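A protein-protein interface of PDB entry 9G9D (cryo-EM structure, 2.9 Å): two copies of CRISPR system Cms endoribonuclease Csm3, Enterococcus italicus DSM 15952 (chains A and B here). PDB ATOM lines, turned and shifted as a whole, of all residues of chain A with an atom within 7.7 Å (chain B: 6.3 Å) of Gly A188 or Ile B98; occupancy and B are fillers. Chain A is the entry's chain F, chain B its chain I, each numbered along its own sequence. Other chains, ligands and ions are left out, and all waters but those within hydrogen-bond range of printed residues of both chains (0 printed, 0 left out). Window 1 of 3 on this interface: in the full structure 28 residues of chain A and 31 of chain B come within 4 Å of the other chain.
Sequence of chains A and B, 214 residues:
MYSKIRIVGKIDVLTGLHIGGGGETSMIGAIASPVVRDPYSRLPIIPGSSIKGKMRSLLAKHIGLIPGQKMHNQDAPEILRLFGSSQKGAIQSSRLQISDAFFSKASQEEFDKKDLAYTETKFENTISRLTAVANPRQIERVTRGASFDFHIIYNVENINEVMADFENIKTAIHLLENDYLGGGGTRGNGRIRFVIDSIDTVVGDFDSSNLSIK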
ATOM      1  N   THR A  15      -1.111  18.568 -10.126  1.00  0.00           N
ATOM      2  CA  THR A  15      -1.134  17.119 -10.014  1.00  0.00           C
ATOM      3  C   THR A  15       0.172  16.583 -10.578  1.00  0.00           C
ATOM      4  O   THR A  15       0.722  17.151 -11.523  1.00  0.00           O
ATOM      5  CB  THR A  15      -2.330  16.519 -10.761  1.00  0.00           C
ATOM      6  OG1 THR A  15      -3.532  17.166 -10.328  1.00  0.00           O
ATOM      7  CG2 THR A  15      -2.450  15.043 -10.477  1.00  0.00           C
ATOM      8  N   GLY A  16       0.656  15.488  -9.995  1.00  0.00           N
ATOM      9  CA  GLY A  16       2.006  15.034 -10.289  1.00  0.00           C
ATOM     10  C   GLY A  16       2.264  14.946 -11.782  1.00  0.00           C
ATOM     11  O   GLY A  16       1.468  14.392 -12.541  1.00  0.00           O
ATOM     12  N   LEU A  17       3.390  15.509 -12.203  1.00  0.00           N
ATOM     13  CA  LEU A  17       3.703  15.703 -13.609  1.00  0.00           C
ATOM     14  C   LEU A  17       4.728  14.676 -14.066  1.00  0.00           C
ATOM     15  O   LEU A  17       5.787  14.526 -13.450  1.00  0.00           O
ATOM     16  CB  LEU A  17       4.239  17.114 -13.846  1.00  0.00           C
ATOM     17  CG  LEU A  17       4.903  17.430 -15.182  1.00  0.00           C
ATOM     18  CD1 LEU A  17       3.864  17.766 -16.218  1.00  0.00           C
ATOM     19  CD2 LEU A  17       5.882  18.572 -15.018  1.00  0.00           C
ATOM     20  N   GLU A 120       8.344  11.677  -6.970  1.00  0.00           N
ATOM     21  CA  GLU A 120       7.718  10.563  -6.279  1.00  0.00           C
ATOM     22  C   GLU A 120       7.575   9.381  -7.228  1.00  0.00           C
ATOM     23  O   GLU A 120       7.391   9.551  -8.435  1.00  0.00           O
ATOM     24  CB  GLU A 120       6.339  10.953  -5.741  1.00  0.00           C
ATOM     25  CG  GLU A 120       5.398  11.475  -6.810  1.00  0.00           C
ATOM     26  CD  GLU A 120       3.973  11.018  -6.603  1.00  0.00           C
ATOM     27  OE1 GLU A 120       3.651  10.553  -5.490  1.00  0.00           O
ATOM     28  OE2 GLU A 120       3.175  11.115  -7.556  1.00  0.00           O
ATOM     29  N   LYS A 122       5.211   6.731  -8.237  1.00  0.00           N
ATOM     30  CA  LYS A 122       3.846   6.241  -8.193  1.00  0.00           C
ATOM     31  C   LYS A 122       3.806   4.772  -8.587  1.00  0.00           C
ATOM     32  O   LYS A 122       4.399   4.364  -9.588  1.00  0.00           O
ATOM     33  CB  LYS A 122       2.962   7.061  -9.129  1.00  0.00           C
ATOM     34  CG  LYS A 122       1.514   6.641  -9.120  1.00  0.00           C
ATOM     35  CD  LYS A 122       0.676   7.553  -9.984  1.00  0.00           C
ATOM     36  CE  LYS A 122      -0.778   7.423  -9.609  1.00  0.00           C
ATOM     37  NZ  LYS A 122      -0.906   7.483  -8.132  1.00  0.00           N
ATOM     38  N   GLU A 124       1.586   1.680  -9.825  1.00  0.00           N
ATOM     39  CA  GLU A 124       0.359   1.415 -10.554  1.00  0.00           C
ATOM     40  C   GLU A 124       0.387  -0.027 -11.027  1.00  0.00           C
ATOM     41  O   GLU A 124       1.417  -0.696 -10.958  1.00  0.00           O
ATOM     42  CB  GLU A 124       0.206   2.369 -11.746  1.00  0.00           C
ATOM     43  CG  GLU A 124       0.572   3.811 -11.445  1.00  0.00           C
ATOM     44  CD  GLU A 124       0.147   4.753 -12.546  1.00  0.00           C
ATOM     45  OE1 GLU A 124      -0.920   4.513 -13.145  1.00  0.00           O
ATOM     46  OE2 GLU A 124       0.877   5.729 -12.820  1.00  0.00           O
ATOM     47  N   ARG A 141       7.108  10.747 -11.057  1.00  0.00           N
ATOM     48  CA  ARG A 141       6.343  11.963 -11.274  1.00  0.00           C
ATOM     49  C   ARG A 141       6.972  13.099 -10.488  1.00  0.00           C
ATOM     50  O   ARG A 141       7.629  12.876  -9.470  1.00  0.00           O
ATOM     51  CB  ARG A 141       4.880  11.802 -10.852  1.00  0.00           C
ATOM     52  CG  ARG A 141       4.135  10.697 -11.570  1.00  0.00           C
ATOM     53  CD  ARG A 141       2.640  10.887 -11.423  1.00  0.00           C
ATOM     54  NE  ARG A 141       2.246  11.100 -10.036  1.00  0.00           N
ATOM     55  CZ  ARG A 141       1.003  11.337  -9.637  1.00  0.00           C
ATOM     56  NH1 ARG A 141       0.002  11.399 -10.497  1.00  0.00           N
ATOM     57  NH2 ARG A 141       0.761  11.515  -8.342  1.00  0.00           N
ATOM     58  N   TYR A 180      -3.766  18.952 -19.485  1.00  0.00           N
ATOM     59  CA  TYR A 180      -2.637  18.413 -18.750  1.00  0.00           C
ATOM     60  C   TYR A 180      -1.367  18.601 -19.564  1.00  0.00           C
ATOM     61  O   TYR A 180      -1.402  18.936 -20.749  1.00  0.00           O
ATOM     62  CB  TYR A 180      -2.845  16.932 -18.413  1.00  0.00           C
ATOM     63  CG  TYR A 180      -3.054  16.037 -19.613  1.00  0.00           C
ATOM     64  CD1 TYR A 180      -1.978  15.443 -20.256  1.00  0.00           C
ATOM     65  CD2 TYR A 180      -4.328  15.773 -20.088  1.00  0.00           C
ATOM     66  CE1 TYR A 180      -2.165  14.620 -21.340  1.00  0.00           C
ATOM     67  CE2 TYR A 180      -4.525  14.951 -21.174  1.00  0.00           C
ATOM     68  CZ  TYR A 180      -3.440  14.377 -21.795  1.00  0.00           C
ATOM     69  OH  TYR A 180      -3.626  13.555 -22.879  1.00  0.00           O
ATOM     70  N   GLY A 183       2.933  13.054 -19.806  1.00  0.00           N
ATOM     71  CA  GLY A 183       2.254  11.797 -20.042  1.00  0.00           C
ATOM     72  C   GLY A 183       1.330  11.408 -18.905  1.00  0.00           C
ATOM     73  O   GLY A 183       1.438  11.894 -17.780  1.00  0.00           O
ATOM     74  N   GLY A 184       0.402  10.506 -19.216  1.00  0.00           N
ATOM     75  CA  GLY A 184      -0.516   9.971 -18.236  1.00  0.00           C
ATOM     76  C   GLY A 184      -1.562  10.938 -17.738  1.00  0.00           C
ATOM     77  O   GLY A 184      -2.262  10.616 -16.771  1.00  0.00           O
ATOM     78  N   GLY A 185      -1.705  12.102 -18.371  1.00  0.00           N
ATOM     79  CA  GLY A 185      -2.594  13.121 -17.836  1.00  0.00           C
ATOM     80  C   GLY A 185      -4.048  12.705 -17.835  1.00  0.00           C
ATOM     81  O   GLY A 185      -4.838  13.175 -17.015  1.00  0.00           O
ATOM     82  N   THR A 186      -4.420  11.797 -18.739  1.00  0.00           N
ATOM     83  CA  THR A 186      -5.819  11.320 -18.797  1.00  0.00           C
ATOM     84  C   THR A 186      -6.152  10.566 -17.524  1.00  0.00           C
ATOM     85  O   THR A 186      -7.352  10.489 -17.184  1.00  0.00           O
ATOM     86  CB  THR A 186      -5.992  10.449 -20.037  1.00  0.00           C
ATOM     87  OG1 THR A 186      -7.365  10.076 -20.003  1.00  0.00           O
ATOM     88  CG2 THR A 186      -5.090   9.228 -20.014  1.00  0.00           C
ATOM     89  N   ARG A 187      -5.141  10.025 -16.840  1.00  0.00           N
ATOM     90  CA  ARG A 187      -5.334   9.271 -15.610  1.00  0.00           C
ATOM     91  C   ARG A 187      -4.912  10.106 -14.409  1.00  0.00           C
ATOM     92  O   ARG A 187      -4.584   9.584 -13.344  1.00  0.00           O
ATOM     93  CB  ARG A 187      -4.572   7.951 -15.653  1.00  0.00           C
ATOM     94  CG  ARG A 187      -5.230   6.898 -16.531  1.00  0.00           C
ATOM     95  CD  ARG A 187      -4.363   5.664 -16.665  1.00  0.00           C
ATOM     96  NE  ARG A 187      -3.063   5.983 -17.242  1.00  0.00           N
ATOM     97  CZ  ARG A 187      -2.823   6.072 -18.541  1.00  0.00           C
ATOM     98  NH1 ARG A 187      -3.776   5.879 -19.434  1.00  0.00           N
ATOM     99  NH2 ARG A 187      -1.594   6.365 -18.955  1.00  0.00           N
ATOM    100  N   GLY A 188      -4.921  11.425 -14.575  1.00  0.00           N
ATOM    101  CA  GLY A 188      -4.605  12.330 -13.490  1.00  0.00           C
ATOM    102  C   GLY A 188      -3.132  12.612 -13.292  1.00  0.00           C
ATOM    103  O   GLY A 188      -2.589  12.365 -12.213  1.00  0.00           O
ATOM    104  N   ASN A 189      -2.477  13.129 -14.324  1.00  0.00           N
ATOM    105  CA  ASN A 189      -1.094  13.563 -14.231  1.00  0.00           C
ATOM    106  C   ASN A 189      -0.943  14.924 -14.889  1.00  0.00           C
ATOM    107  O   ASN A 189      -1.724  15.299 -15.766  1.00  0.00           O
ATOM    108  CB  ASN A 189      -0.130  12.572 -14.899  1.00  0.00           C
ATOM    109  CG  ASN A 189       0.115  11.339 -14.061  1.00  0.00           C
ATOM    110  OD1 ASN A 189      -0.134  11.334 -12.860  1.00  0.00           O
ATOM    111  ND2 ASN A 189       0.620  10.286 -14.692  1.00  0.00           N
ATOM    112  N   GLY A 190       0.056  15.673 -14.436  1.00  0.00           N
ATOM    113  CA  GLY A 190       0.519  16.828 -15.171  1.00  0.00           C
ATOM    114  C   GLY A 190      -0.384  18.036 -15.164  1.00  0.00           C
ATOM    115  O   GLY A 190      -0.146  18.959 -15.950  1.00  0.00           O
ATOM    116  N   ARG A 191      -1.416  18.070 -14.325  1.00  0.00           N
ATOM    117  CA  ARG A 191      -2.232  19.271 -14.236  1.00  0.00           C
ATOM    118  C   ARG A 191      -1.391  20.424 -13.711  1.00  0.00           C
ATOM    119  O   ARG A 191      -0.688  20.295 -12.707  1.00  0.00           O
ATOM    120  CB  ARG A 191      -3.438  19.040 -13.330  1.00  0.00           C
ATOM    121  CG  ARG A 191      -4.369  17.953 -13.817  1.00  0.00           C
ATOM    122  CD  ARG A 191      -5.810  18.238 -13.427  1.00  0.00           C
ATOM    123  NE  ARG A 191      -5.953  18.610 -12.025  1.00  0.00           N
ATOM    124  CZ  ARG A 191      -6.176  19.846 -11.600  1.00  0.00           C
ATOM    125  NH1 ARG A 191      -6.279  20.858 -12.444  1.00  0.00           N
ATOM    126  NH2 ARG A 191      -6.302  20.071 -10.295  1.00  0.00           N
ATOM    127  N   PRO B  47      -5.819   8.068  -6.291  1.00  0.00           N
ATOM    128  CA  PRO B  47      -5.193   8.313  -7.580  1.00  0.00           C
ATOM    129  C   PRO B  47      -6.217   8.396  -8.695  1.00  0.00           C
ATOM    130  O   PRO B  47      -7.199   7.637  -8.678  1.00  0.00           O
ATOM    131  CB  PRO B  47      -4.257   7.110  -7.730  1.00  0.00           C
ATOM    132  CG  PRO B  47      -4.080   6.605  -6.320  1.00  0.00           C
ATOM    133  CD  PRO B  47      -5.453   6.796  -5.711  1.00  0.00           C
ATOM    134  N   GLY B  48      -5.976   9.274  -9.668  1.00  0.00           N
ATOM    135  CA  GLY B  48      -6.886   9.390 -10.820  1.00  0.00           C
ATOM    136  C   GLY B  48      -6.903   8.089 -11.587  1.00  0.00           C
ATOM    137  O   GLY B  48      -7.991   7.681 -12.038  1.00  0.00           O
ATOM    138  N   SER B  49      -5.734   7.459 -11.725  1.00  0.00           N
ATOM    139  CA  SER B  49      -5.627   6.188 -12.481  1.00  0.00           C
ATOM    140  C   SER B  49      -6.479   5.116 -11.799  1.00  0.00           C
ATOM    141  O   SER B  49      -7.143   4.343 -12.518  1.00  0.00           O
ATOM    142  CB  SER B  49      -4.198   5.749 -12.548  1.00  0.00           C
ATOM    143  OG  SER B  49      -3.644   5.638 -11.246  1.00  0.00           O
ATOM    144  N   ILE B  51      -9.198   5.508  -9.923  1.00  0.00           N
ATOM    145  CA  ILE B  51     -10.639   5.764 -10.215  1.00  0.00           C
ATOM    146  C   ILE B  51     -10.948   5.398 -11.674  1.00  0.00           C
ATOM    147  O   ILE B  51     -11.959   4.710 -11.907  1.00  0.00           O
ATOM    148  CB  ILE B  51     -10.997   7.235  -9.936  1.00  0.00           C
ATOM    149  CG1 ILE B  51     -10.376   7.735  -8.637  1.00  0.00           C
ATOM    150  CG2 ILE B  51     -12.511   7.443  -9.951  1.00  0.00           C
ATOM    151  CD1 ILE B  51     -10.375   9.246  -8.495  1.00  0.00           C
ATOM    152  N   LYS B  52     -10.079   5.800 -12.604  1.00  0.00           N
ATOM    153  CA  LYS B  52     -10.387   5.546 -14.032  1.00  0.00           C
ATOM    154  C   LYS B  52     -10.413   4.037 -14.290  1.00  0.00           C
ATOM    155  O   LYS B  52     -11.351   3.563 -14.956  1.00  0.00           O
ATOM    156  CB  LYS B  52      -9.346   6.231 -14.923  1.00  0.00           C
ATOM    157  CG  LYS B  52      -9.746   6.362 -16.384  1.00  0.00           C
ATOM    158  CD  LYS B  52      -8.711   7.066 -17.252  1.00  0.00           C
ATOM    159  CE  LYS B  52      -9.152   7.212 -18.671  1.00  0.00           C
ATOM    160  NZ  LYS B  52      -8.020   7.463 -19.567  1.00  0.00           N
ATOM    161  N   MET B  55     -13.486   2.474 -12.798  1.00  0.00           N
ATOM    162  CA  MET B  55     -14.706   2.898 -13.530  1.00  0.00           C
ATOM    163  C   MET B  55     -14.717   2.206 -14.897  1.00  0.00           C
ATOM    164  O   MET B  55     -15.751   1.607 -15.252  1.00  0.00           O
ATOM    165  CB  MET B  55     -14.744   4.415 -13.727  1.00  0.00           C
ATOM    166  CG  MET B  55     -15.201   5.180 -12.504  1.00  0.00           C
ATOM    167  SD  MET B  55     -15.017   6.961 -12.706  1.00  0.00           S
ATOM    168  CE  MET B  55     -16.008   7.215 -14.184  1.00  0.00           C
ATOM    169  N   PHE B  83     -12.864   6.416 -22.728  1.00  0.00           N
ATOM    170  CA  PHE B  83     -11.639   6.262 -21.956  1.00  0.00           C
ATOM    171  C   PHE B  83     -10.385   6.192 -22.816  1.00  0.00           C
ATOM    172  O   PHE B  83      -9.282   6.123 -22.270  1.00  0.00           O
ATOM    173  CB  PHE B  83     -11.727   5.013 -21.074  1.00  0.00           C
ATOM    174  CG  PHE B  83     -12.721   5.129 -19.957  1.00  0.00           C
ATOM    175  CD1 PHE B  83     -12.350   5.655 -18.734  1.00  0.00           C
ATOM    176  CD2 PHE B  83     -14.026   4.707 -20.128  1.00  0.00           C
ATOM    177  CE1 PHE B  83     -13.262   5.762 -17.706  1.00  0.00           C
ATOM    178  CE2 PHE B  83     -14.941   4.812 -19.105  1.00  0.00           C
ATOM    179  CZ  PHE B  83     -14.558   5.340 -17.893  1.00  0.00           C
ATOM    180  N   LEU B  96     -12.151  11.503 -21.074  1.00  0.00           N
ATOM    181  CA  LEU B  96     -12.097  11.682 -19.632  1.00  0.00           C
ATOM    182  C   LEU B  96     -10.670  11.964 -19.190  1.00  0.00           C
ATOM    183  O   LEU B  96      -9.726  11.324 -19.657  1.00  0.00           O
ATOM    184  CB  LEU B  96     -12.631  10.448 -18.904  1.00  0.00           C
ATOM    185  CG  LEU B  96     -14.147  10.268 -18.897  1.00  0.00           C
ATOM    186  CD1 LEU B  96     -14.544   9.083 -18.040  1.00  0.00           C
ATOM    187  CD2 LEU B  96     -14.825  11.532 -18.408  1.00  0.00           C
ATOM    188  N   GLN B  97     -10.523  12.930 -18.290  1.00  0.00           N
ATOM    189  CA  GLN B  97      -9.241  13.289 -17.692  1.00  0.00           C
ATOM    190  C   GLN B  97      -9.346  13.270 -16.175  1.00  0.00           C
ATOM    191  O   GLN B  97      -8.994  14.233 -15.490  1.00  0.00           O
ATOM    192  CB  GLN B  97      -8.760  14.649 -18.176  1.00  0.00           C
ATOM    193  CG  GLN B  97      -8.441  14.698 -19.650  1.00  0.00           C
ATOM    194  CD  GLN B  97      -7.756  15.984 -20.038  1.00  0.00           C
ATOM    195  OE1 GLN B  97      -7.361  16.771 -19.180  1.00  0.00           O
ATOM    196  NE2 GLN B  97      -7.609  16.208 -21.337  1.00  0.00           N
ATOM    197  N   ILE B  98      -9.884  12.171 -15.642  1.00  0.00           N
ATOM    198  CA  ILE B  98     -10.013  12.004 -14.201  1.00  0.00           C
ATOM    199  C   ILE B  98      -8.670  12.256 -13.539  1.00  0.00           C
ATOM    200  O   ILE B  98      -7.636  11.762 -13.999  1.00  0.00           O
ATOM    201  CB  ILE B  98     -10.545  10.597 -13.883  1.00  0.00           C
ATOM    202  CG1 ILE B  98     -11.736  10.275 -14.787  1.00  0.00           C
ATOM    203  CG2 ILE B  98     -10.937  10.501 -12.422  1.00  0.00           C
ATOM    204  CD1 ILE B  98     -12.326   8.909 -14.568  1.00  0.00           C
ATOM    205  N   SER B  99      -8.680  13.037 -12.463  1.00  0.00           N
ATOM    206  CA  SER B  99      -7.462  13.486 -11.806  1.00  0.00           C
ATOM    207  C   SER B  99      -7.441  13.022 -10.357  1.00  0.00           C
ATOM    208  O   SER B  99      -8.437  12.537  -9.815  1.00  0.00           O
ATOM    209  CB  SER B  99      -7.328  15.013 -11.874  1.00  0.00           C
ATOM    210  OG  SER B  99      -8.382  15.652 -11.179  1.00  0.00           O
ATOM    211  N   ASP B 100      -6.273  13.176  -9.734  1.00  0.00           N
ATOM    212  CA  ASP B 100      -6.092  12.764  -8.349  1.00  0.00           C
ATOM    213  C   ASP B 100      -7.047  13.518  -7.434  1.00  0.00           C
ATOM    214  O   ASP B 100      -7.161  14.743  -7.510  1.00  0.00           O
ATOM    215  CB  ASP B 100      -4.649  13.004  -7.914  1.00  0.00           C
ATOM    216  CG  ASP B 100      -3.651  12.263  -8.776  1.00  0.00           C
ATOM    217  OD1 ASP B 100      -4.085  11.550  -9.703  1.00  0.00           O
ATOM    218  OD2 ASP B 100      -2.435  12.393  -8.531  1.00  0.00           O
ATOM    219  N   PHE B 150     -12.651  15.507  -6.322  1.00  0.00           N
ATOM    220  CA  PHE B 150     -12.097  15.125  -7.610  1.00  0.00           C
ATOM    221  C   PHE B 150     -12.256  16.253  -8.622  1.00  0.00           C
ATOM    222  O   PHE B 150     -12.842  17.300  -8.347  1.00  0.00           O
ATOM    223  CB  PHE B 150     -12.759  13.842  -8.123  1.00  0.00           C
ATOM    224  CG  PHE B 150     -14.232  13.976  -8.393  1.00  0.00           C
ATOM    225  CD1 PHE B 150     -14.691  14.344  -9.646  1.00  0.00           C
ATOM    226  CD2 PHE B 150     -15.158  13.710  -7.402  1.00  0.00           C
ATOM    227  CE1 PHE B 150     -16.044  14.458  -9.900  1.00  0.00           C
ATOM    228  CE2 PHE B 150     -16.513  13.822  -7.652  1.00  0.00           C
ATOM    229  CZ  PHE B 150     -16.955  14.197  -8.903  1.00  0.00           C
ATOM    230  N   HIS B 151     -11.713  16.016  -9.816  1.00  0.00           N
ATOM    231  CA  HIS B 151     -11.736  17.002 -10.894  1.00  0.00           C
ATOM    232  C   HIS B 151     -11.644  16.230 -12.207  1.00  0.00           C
ATOM    233  O   HIS B 151     -10.561  15.771 -12.582  1.00  0.00           O
ATOM    234  CB  HIS B 151     -10.595  17.998 -10.744  1.00  0.00           C
ATOM    235  CG  HIS B 151     -10.441  18.925 -11.909  1.00  0.00           C
ATOM    236  ND1 HIS B 151      -9.249  19.548 -12.211  1.00  0.00           N
ATOM    237  CD2 HIS B 151     -11.328  19.338 -12.845  1.00  0.00           C
ATOM    238  CE1 HIS B 151      -9.409  20.301 -13.284  1.00  0.00           C
ATOM    239  NE2 HIS B 151     -10.661  20.191 -13.688  1.00  0.00           N
ATOM    240  N   ILE B 152     -12.773  16.090 -12.894  1.00  0.00           N
ATOM    241  CA  ILE B 152     -12.854  15.327 -14.135  1.00  0.00           C
ATOM    242  C   ILE B 152     -13.077  16.300 -15.283  1.00  0.00           C
ATOM    243  O   ILE B 152     -14.067  17.040 -15.296  1.00  0.00           O
ATOM    244  CB  ILE B 152     -13.973  14.278 -14.082  1.00  0.00           C
ATOM    245  CG1 ILE B 152     -13.729  13.289 -12.941  1.00  0.00           C
ATOM    246  CG2 ILE B 152     -14.068  13.548 -15.402  1.00  0.00           C
ATOM    247  CD1 ILE B 152     -14.805  12.232 -12.807  1.00  0.00           C
ATOM    248  N   ILE B 153     -12.167  16.296 -16.251  1.00  0.00           N
ATOM    249  CA  ILE B 153     -12.292  17.111 -17.454  1.00  0.00           C
ATOM    250  C   ILE B 153     -12.838  16.239 -18.574  1.00  0.00           C
ATOM    251  O   ILE B 153     -12.327  15.141 -18.826  1.00  0.00           O
ATOM    252  CB  ILE B 153     -10.945  17.738 -17.851  1.00  0.00           C
ATOM    253  CG1 ILE B 153     -10.637  18.952 -16.974  1.00  0.00           C
ATOM    254  CG2 ILE B 153     -10.955  18.151 -19.311  1.00  0.00           C
ATOM    255  CD1 ILE B 153     -11.621  20.086 -17.141  1.00  0.00           C
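Among the printed residues, merely in contact across the chains: Arg A187 with Ile B98 (3.2 Å), Arg A187 with Gly B48 (3.3 Å), Thr A15 with Asp B100 (3.3 Å), Tyr A180 with Gln B97 (3.3 Å), Lys A122 with Pro B47 (3.4 Å), Thr A186 with Gln B97 (3.4 Å), Glu A124 with Ser B49 (3.5 Å), Gly A188 with Ser B99 (3.5 Å), Arg A187 with Lys B52 (3.6 Å), Lys A122 with Ser B49 (3.8 Å) and Arg A191 with Ser B99 (3.9 Å).
No position is printed for both chains.
NH1 of Arg A141 is in salt-bridge range of OD2 of Asp B100, at 3.3 Å.
NZ of Lys B52 sits at hydrogen-bond distance from OG1 of Thr A186, at 2.7 Å.
The backbone carbonyl oxygen of Leu B96 lies within hydrogen-bond range of the side-chain hydroxyl of Thr A186 (2.7 Å).
N of Ile B98 sits at hydrogen-bond distance from O of Thr A186 (3.4 Å).
The backbone carbonyl oxygen of Arg A187 is in hydrogen-bond range of the backbone NH of Ser B49 (2.9 Å).
The backbone NH (N) of Gly A188 is in hydrogen-bond range of the backbone carbonyl oxygen (O) of Ile B98 (2.8 Å).
The guanidinium group (NH1) of Arg A191 lies close to a ring nitrogen (ND1) of His B151, 3.3 Å away.
The backbone carbonyl oxygen (O) of Gly A188 sits close to the side-chain carboxylate (OD1) of Asp B100 (3.0 Å).
Of chain B, only Ile B98 (2.8 Å), Ser B99 (3.5 Å) and Asp B100 (3.0 Å) come within 4 Å of Gly A188.
Of chain A, only Thr A186 (3.4 Å), Arg A187 (3.2 Å) and Gly A188 (2.8 Å) come within 4 Å of Ile B98.
Of the printed residues of chain B, Thr A186 touches Lys B52 (2.7 Å), Leu B96 (2.7 Å), Gln B97 (3.4 Å) and Ile B98 (3.4 Å).
Of the printed residues of chain A, Ser B99 touches Gly A188 (3.5 Å) and Arg A191 (3.9 Å).
The nearest residue of chain B that does not touch Gly A188 is Gly B48 (4.6 Å).
The nearest residue of chain A that does not touch Ile B98 is Gly A185 (4.3 Å).
The nearest printed residue of chain A that does not touch Leu B96 is Arg A187 (5.5 Å).
The backbone carbonyl oxygen (O) of Arg A191 is in hydrogen-bond range of the backbone NH (N) of Thr A15 (3.1 Å).
OE2 of Glu A120 lies within salt-bridge range of NH2 of Arg A141 (2.6 Å).
The backbone carbonyl oxygen of Gly A188 sits at hydrogen-bond distance from the guanidinium group of Arg A141 (3.3 Å).
N of Gly B48 sits at hydrogen-bond distance from OD1 of Asp B100, 3.0 Å away.
The side-chain amino group of Lys B52 lies within hydrogen-bond range of the backbone carbonyl oxygen of Phe B83.
N of Gln B97 sits at hydrogen-bond distance from O of Ile B153 (2.9 Å).
Of the 17 printed residues of chain A, 9 touch a printed residue of chain B.
Hydrophobic or aromatic side chains of chain A within 4 Å of the printed part of chain B: Tyr A180.
Printed residues of chain B that touch a printed residue of chain A: Pro B47, Gly B48, Ser B49, Lys B52, Leu B96, Gln B97, Ile B98, Ser B99, Asp B100 and His B151.
Hydrophobic or aromatic side chains of chain B that line the printed part of chain A: Pro B47 and His B151.
Among the printed residues, 19 pairs touch across the chains.
Among the printed residues, Asp or Glu carboxylates within 4 Å of a Lys or Arg side-chain nitrogen of the other chain: Arg A141 with Asp B100 (3.3 Å).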
